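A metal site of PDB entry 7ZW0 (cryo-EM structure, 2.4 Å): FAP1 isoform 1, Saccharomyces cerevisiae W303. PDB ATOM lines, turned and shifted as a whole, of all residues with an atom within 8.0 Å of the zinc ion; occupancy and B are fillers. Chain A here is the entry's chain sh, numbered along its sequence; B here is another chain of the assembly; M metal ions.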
ATOM      1  N   MET A 182       9.237 -18.141  -7.804  1.00  0.00           N
ATOM      2  CA  MET A 182       9.235 -17.689  -9.191  1.00  0.00           C
ATOM      3  C   MET A 182       9.904 -18.590 -10.226  1.00  0.00           C
ATOM      4  O   MET A 182      10.729 -19.435  -9.862  1.00  0.00           O
ATOM      5  CB  MET A 182       9.873 -16.300  -9.297  1.00  0.00           C
ATOM      6  CG  MET A 182       8.946 -15.134  -9.021  1.00  0.00           C
ATOM      7  SD  MET A 182       9.845 -13.578  -8.911  1.00  0.00           S
ATOM      8  CE  MET A 182      10.642 -13.761  -7.321  1.00  0.00           C
ATOM      9  N   CYS A 183       9.531 -18.437 -11.496  1.00  0.00           N
ATOM     10  CA  CYS A 183      10.146 -19.206 -12.582  1.00  0.00           C
ATOM     11  C   CYS A 183      11.607 -18.804 -12.800  1.00  0.00           C
ATOM     12  O   CYS A 183      12.041 -17.761 -12.296  1.00  0.00           O
ATOM     13  CB  CYS A 183       9.299 -19.043 -13.855  1.00  0.00           C
ATOM     14  SG  CYS A 183       9.513 -17.383 -14.560  1.00  0.00           S
ATOM     15  N   HIS A 184      12.396 -19.564 -13.557  1.00  0.00           N
ATOM     16  CA  HIS A 184      13.837 -19.288 -13.715  1.00  0.00           C
ATOM     17  C   HIS A 184      14.193 -17.855 -14.155  1.00  0.00           C
ATOM     18  O   HIS A 184      15.198 -17.333 -13.688  1.00  0.00           O
ATOM     19  CB  HIS A 184      14.440 -20.240 -14.751  1.00  0.00           C
ATOM     20  CG  HIS A 184      14.355 -21.680 -14.361  1.00  0.00           C
ATOM     21  ND1 HIS A 184      14.949 -22.241 -13.267  1.00  0.00           N
ATOM     22  CD2 HIS A 184      13.748 -22.686 -15.067  1.00  0.00           C
ATOM     23  CE1 HIS A 184      14.745 -23.555 -13.318  1.00  0.00           C
ATOM     24  NE2 HIS A 184      14.012 -23.888 -14.396  1.00  0.00           N
ATOM     25  N   CYS A 185      13.385 -17.231 -15.016  1.00  0.00           N
ATOM     26  CA  CYS A 185      13.611 -15.861 -15.480  1.00  0.00           C
ATOM     27  C   CYS A 185      12.962 -14.778 -14.603  1.00  0.00           C
ATOM     28  O   CYS A 185      13.180 -13.595 -14.866  1.00  0.00           O
ATOM     29  CB  CYS A 185      13.179 -15.749 -16.951  1.00  0.00           C
ATOM     30  SG  CYS A 185      11.380 -15.943 -17.113  1.00  0.00           S
ATOM     31  N   GLY A 186      12.168 -15.161 -13.599  1.00  0.00           N
ATOM     32  CA  GLY A 186      11.521 -14.246 -12.661  1.00  0.00           C
ATOM     33  C   GLY A 186      10.226 -13.592 -13.162  1.00  0.00           C
ATOM     34  O   GLY A 186       9.585 -12.881 -12.400  1.00  0.00           O
ATOM     35  N   LYS A 187       9.791 -13.849 -14.408  1.00  0.00           N
ATOM     36  CA  LYS A 187       8.600 -13.206 -14.989  1.00  0.00           C
ATOM     37  C   LYS A 187       7.272 -13.625 -14.351  1.00  0.00           C
ATOM     38  O   LYS A 187       6.317 -12.868 -14.397  1.00  0.00           O
ATOM     39  CB  LYS A 187       8.526 -13.500 -16.493  1.00  0.00           C
ATOM     40  CG  LYS A 187       9.606 -12.808 -17.324  1.00  0.00           C
ATOM     41  CD  LYS A 187       9.350 -13.158 -18.804  1.00  0.00           C
ATOM     42  CE  LYS A 187      10.386 -12.583 -19.763  1.00  0.00           C
ATOM     43  NZ  LYS A 187      10.038 -12.971 -21.158  1.00  0.00           N
ATOM     44  N   HIS A 188       7.197 -14.863 -13.855  1.00  0.00           N
ATOM     45  CA  HIS A 188       5.940 -15.375 -13.315  1.00  0.00           C
ATOM     46  C   HIS A 188       6.125 -16.081 -11.997  1.00  0.00           C
ATOM     47  O   HIS A 188       7.181 -16.633 -11.722  1.00  0.00           O
ATOM     48  CB  HIS A 188       5.289 -16.329 -14.312  1.00  0.00           C
ATOM     49  CG  HIS A 188       4.843 -15.667 -15.575  1.00  0.00           C
ATOM     50  ND1 HIS A 188       3.908 -14.663 -15.585  1.00  0.00           N
ATOM     51  CD2 HIS A 188       5.235 -15.831 -16.859  1.00  0.00           C
ATOM     52  CE1 HIS A 188       3.718 -14.259 -16.825  1.00  0.00           C
ATOM     53  NE2 HIS A 188       4.514 -14.946 -17.619  1.00  0.00           N
ATOM     54  N   SER A 189       5.089 -16.063 -11.175  1.00  0.00           N
ATOM     55  CA  SER A 189       5.167 -16.692  -9.866  1.00  0.00           C
ATOM     56  C   SER A 189       4.252 -17.895  -9.764  1.00  0.00           C
ATOM     57  O   SER A 189       3.413 -18.124 -10.636  1.00  0.00           O
ATOM     58  CB  SER A 189       4.840 -15.672  -8.785  1.00  0.00           C
ATOM     59  OG  SER A 189       3.557 -15.115  -8.978  1.00  0.00           O
ATOM     60  N   PHE A 204       9.921 -25.137 -10.956  1.00  0.00           N
ATOM     61  CA  PHE A 204       9.222 -24.079 -11.694  1.00  0.00           C
ATOM     62  C   PHE A 204       9.982 -23.419 -12.842  1.00  0.00           C
ATOM     63  O   PHE A 204      11.124 -22.983 -12.669  1.00  0.00           O
ATOM     64  CB  PHE A 204       8.591 -23.026 -10.763  1.00  0.00           C
ATOM     65  CG  PHE A 204       7.488 -22.238 -11.409  1.00  0.00           C
ATOM     66  CD1 PHE A 204       6.581 -22.853 -12.254  1.00  0.00           C
ATOM     67  CD2 PHE A 204       7.355 -20.889 -11.179  1.00  0.00           C
ATOM     68  CE1 PHE A 204       5.570 -22.119 -12.866  1.00  0.00           C
ATOM     69  CE2 PHE A 204       6.361 -20.151 -11.789  1.00  0.00           C
ATOM     70  CZ  PHE A 204       5.459 -20.770 -12.627  1.00  0.00           C
ATOM     71  N   ASN A 205       9.350 -23.324 -13.994  1.00  0.00           N
ATOM     72  CA  ASN A 205       9.966 -22.743 -15.178  1.00  0.00           C
ATOM     73  C   ASN A 205       8.797 -22.126 -15.921  1.00  0.00           C
ATOM     74  O   ASN A 205       7.849 -22.845 -16.247  1.00  0.00           O
ATOM     75  CB  ASN A 205      10.531 -23.902 -16.012  1.00  0.00           C
ATOM     76  CG  ASN A 205      11.385 -23.449 -17.185  1.00  0.00           C
ATOM     77  OD1 ASN A 205      11.278 -22.324 -17.647  1.00  0.00           O
ATOM     78  ND2 ASN A 205      12.224 -24.344 -17.676  1.00  0.00           N
ATOM     79  N   CYS A 206       8.813 -20.817 -16.199  1.00  0.00           N
ATOM     80  CA  CYS A 206       7.690 -20.297 -16.978  1.00  0.00           C
ATOM     81  C   CYS A 206       7.761 -20.762 -18.416  1.00  0.00           C
ATOM     82  O   CYS A 206       6.721 -21.029 -19.024  1.00  0.00           O
ATOM     83  CB  CYS A 206       7.528 -18.774 -16.883  1.00  0.00           C
ATOM     84  SG  CYS A 206       8.566 -17.774 -17.976  1.00  0.00           S
ATOM     85  N   GLN A 207       8.971 -20.832 -18.972  1.00  0.00           N
ATOM     86  CA  GLN A 207       9.194 -21.255 -20.373  1.00  0.00           C
ATOM     87  C   GLN A 207       8.929 -20.186 -21.417  1.00  0.00           C
ATOM     88  O   GLN A 207       8.957 -20.460 -22.611  1.00  0.00           O
ATOM     89  CB  GLN A 207       8.560 -22.629 -20.720  1.00  0.00           C
ATOM     90  CG  GLN A 207       9.045 -23.744 -19.803  1.00  0.00           C
ATOM     91  CD  GLN A 207       9.196 -25.081 -20.499  1.00  0.00           C
ATOM     92  OE1 GLN A 207       8.747 -25.272 -21.625  1.00  0.00           O
ATOM     93  NE2 GLN A 207       9.834 -26.025 -19.817  1.00  0.00           N
ATOM     94  N   GLU A 208       8.688 -18.950 -20.987  1.00  0.00           N
ATOM     95  CA  GLU A 208       8.566 -17.879 -21.953  1.00  0.00           C
ATOM     96  C   GLU A 208       9.986 -17.646 -22.460  1.00  0.00           C
ATOM     97  O   GLU A 208      10.912 -17.643 -21.661  1.00  0.00           O
ATOM     98  CB  GLU A 208       7.980 -16.606 -21.337  1.00  0.00           C
ATOM     99  CG  GLU A 208       6.498 -16.750 -21.013  1.00  0.00           C
ATOM    100  CD  GLU A 208       5.828 -15.448 -20.623  1.00  0.00           C
ATOM    101  OE1 GLU A 208       4.589 -15.444 -20.494  1.00  0.00           O
ATOM    102  OE2 GLU A 208       6.535 -14.437 -20.441  1.00  0.00           O
ATOM    103  N   VAL A 209      10.154 -17.416 -23.746  1.00  0.00           N
ATOM    104  CA  VAL A 209      11.506 -17.299 -24.303  1.00  0.00           C
ATOM    105  C   VAL A 209      12.283 -16.173 -23.645  1.00  0.00           C
ATOM    106  O   VAL A 209      11.710 -15.109 -23.387  1.00  0.00           O
ATOM    107  CB  VAL A 209      11.406 -17.001 -25.809  1.00  0.00           C
ATOM    108  CG1 VAL A 209      12.771 -16.972 -26.484  1.00  0.00           C
ATOM    109  CG2 VAL A 209      10.499 -18.015 -26.494  1.00  0.00           C
ATOM    110  N   CYS A 210      13.571 -16.386 -23.376  1.00  0.00           N
ATOM    111  CA  CYS A 210      14.368 -15.363 -22.736  1.00  0.00           C
ATOM    112  C   CYS A 210      14.377 -14.150 -23.633  1.00  0.00           C
ATOM    113  O   CYS A 210      14.148 -13.036 -23.168  1.00  0.00           O
ATOM    114  CB  CYS A 210      15.783 -15.876 -22.572  1.00  0.00           C
ATOM    115  SG  CYS A 210      16.912 -14.736 -21.764  1.00  0.00           S
ATOM    116  N   LYS A 224      14.268 -20.601 -23.943  1.00  0.00           N
ATOM    117  CA  LYS A 224      13.088 -20.329 -23.127  1.00  0.00           C
ATOM    118  C   LYS A 224      13.566 -19.884 -21.768  1.00  0.00           C
ATOM    119  O   LYS A 224      14.760 -19.835 -21.529  1.00  0.00           O
ATOM    120  CB  LYS A 224      12.275 -21.600 -22.950  1.00  0.00           C
ATOM    121  CG  LYS A 224      11.568 -22.104 -24.189  1.00  0.00           C
ATOM    122  CD  LYS A 224      10.692 -23.295 -23.828  1.00  0.00           C
ATOM    123  CE  LYS A 224       9.762 -23.704 -24.953  1.00  0.00           C
ATOM    124  NZ  LYS A 224       8.799 -24.749 -24.506  1.00  0.00           N
ATOM    125  N   CYS A 225      12.657 -19.539 -20.870  1.00  0.00           N
ATOM    126  CA  CYS A 225      13.063 -19.043 -19.565  1.00  0.00           C
ATOM    127  C   CYS A 225      14.001 -20.060 -18.979  1.00  0.00           C
ATOM    128  O   CYS A 225      13.712 -21.258 -18.964  1.00  0.00           O
ATOM    129  CB  CYS A 225      11.843 -18.891 -18.683  1.00  0.00           C
ATOM    130  SG  CYS A 225      12.069 -19.324 -16.946  1.00  0.00           S
ATOM    131  N   HIS A 226      15.143 -19.595 -18.504  1.00  0.00           N
ATOM    132  CA  HIS A 226      16.146 -20.528 -18.011  1.00  0.00           C
ATOM    133  C   HIS A 226      16.931 -19.923 -16.868  1.00  0.00           C
ATOM    134  O   HIS A 226      17.037 -18.705 -16.757  1.00  0.00           O
ATOM    135  CB  HIS A 226      17.103 -20.892 -19.147  1.00  0.00           C
ATOM    136  CG  HIS A 226      17.742 -19.714 -19.814  1.00  0.00           C
ATOM    137  ND1 HIS A 226      18.789 -19.024 -19.245  1.00  0.00           N
ATOM    138  CD2 HIS A 226      17.489 -19.101 -20.997  1.00  0.00           C
ATOM    139  CE1 HIS A 226      19.143 -18.034 -20.047  1.00  0.00           C
ATOM    140  NE2 HIS A 226      18.372 -18.057 -21.119  1.00  0.00           N
ATOM    141  N   PRO A 227      17.464 -20.784 -15.990  1.00  0.00           N
ATOM    142  CA  PRO A 227      18.326 -20.218 -14.949  1.00  0.00           C
ATOM    143  C   PRO A 227      19.657 -19.812 -15.583  1.00  0.00           C
ATOM    144  O   PRO A 227      20.117 -20.468 -16.516  1.00  0.00           O
ATOM    145  CB  PRO A 227      18.515 -21.390 -13.997  1.00  0.00           C
ATOM    146  CG  PRO A 227      18.316 -22.616 -14.819  1.00  0.00           C
ATOM    147  CD  PRO A 227      17.378 -22.257 -15.932  1.00  0.00           C
ATOM    148  N   GLN B 117      15.425  -8.169 -10.436  1.00  0.00           N
ATOM    149  CA  GLN B 117      15.356  -9.321 -11.325  1.00  0.00           C
ATOM    150  C   GLN B 117      16.746  -9.891 -11.587  1.00  0.00           C
ATOM    151  O   GLN B 117      16.894 -11.104 -11.768  1.00  0.00           O
ATOM    152  CB  GLN B 117      14.654  -8.943 -12.631  1.00  0.00           C
ATOM    153  CG  GLN B 117      14.244 -10.148 -13.474  1.00  0.00           C
ATOM    154  CD  GLN B 117      13.779 -11.323 -12.639  1.00  0.00           C
ATOM    155  OE1 GLN B 117      14.355 -12.412 -12.699  1.00  0.00           O
ATOM    156  NE2 GLN B 117      12.695 -11.140 -11.883  1.00  0.00           N
ATOM    157  N   HIS B 120      17.310 -11.955  -8.541  1.00  0.00           N
ATOM    158  CA  HIS B 120      16.581 -13.213  -8.658  1.00  0.00           C
ATOM    159  C   HIS B 120      17.238 -14.163  -9.653  1.00  0.00           C
ATOM    160  O   HIS B 120      17.299 -15.373  -9.414  1.00  0.00           O
ATOM    161  CB  HIS B 120      15.139 -12.932  -9.057  1.00  0.00           C
ATOM    162  CG  HIS B 120      14.339 -14.161  -9.325  1.00  0.00           C
ATOM    163  ND1 HIS B 120      14.050 -15.097  -8.348  1.00  0.00           N
ATOM    164  CD2 HIS B 120      13.760 -14.627 -10.466  1.00  0.00           C
ATOM    165  CE1 HIS B 120      13.333 -16.069  -8.870  1.00  0.00           C
ATOM    166  NE2 HIS B 120      13.146 -15.810 -10.152  1.00  0.00           N
HETATM  167 ZN    ZN M   1      10.398 -17.883 -16.655  1.00  0.00          ZN
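SG of Cys 206 lies close to N of Glu 208 (3.2 Å).
N of His 184 sits close to SG of Cys 225 (3.4 Å).
O of Cys 185 sits close to OE1 of Gln 117 of chain B (2.7 Å).
The backbone carbonyl oxygen of Glu 208 lies within hydrogen-bond range of the backbone NH of Cys 225, at 2.7 Å.
SG of Cys 185 lies close to N of Lys 187 (3.8 Å).
N of Gly 186 sits close to SG of Cys 183 (3.6 Å).
The backbone carbonyl oxygen (O) of Cys 225 sits close to the side-chain amide oxygen (OD1) of Asn 205, 3.0 Å away.
O of His 188 is in hydrogen-bond range of N of Cys 183 (3.0 Å).
The zinc ion is bound by SG of Cys 185 (2.2 Å), SG of Cys 225 (2.2 Å), SG of Cys 206 (2.3 Å) and SG of Cys 183 (2.3 Å).
Four residues have an atom within 4 Å of the zinc ion: Cys 183, Cys 185, Cys 206 and Cys 225.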
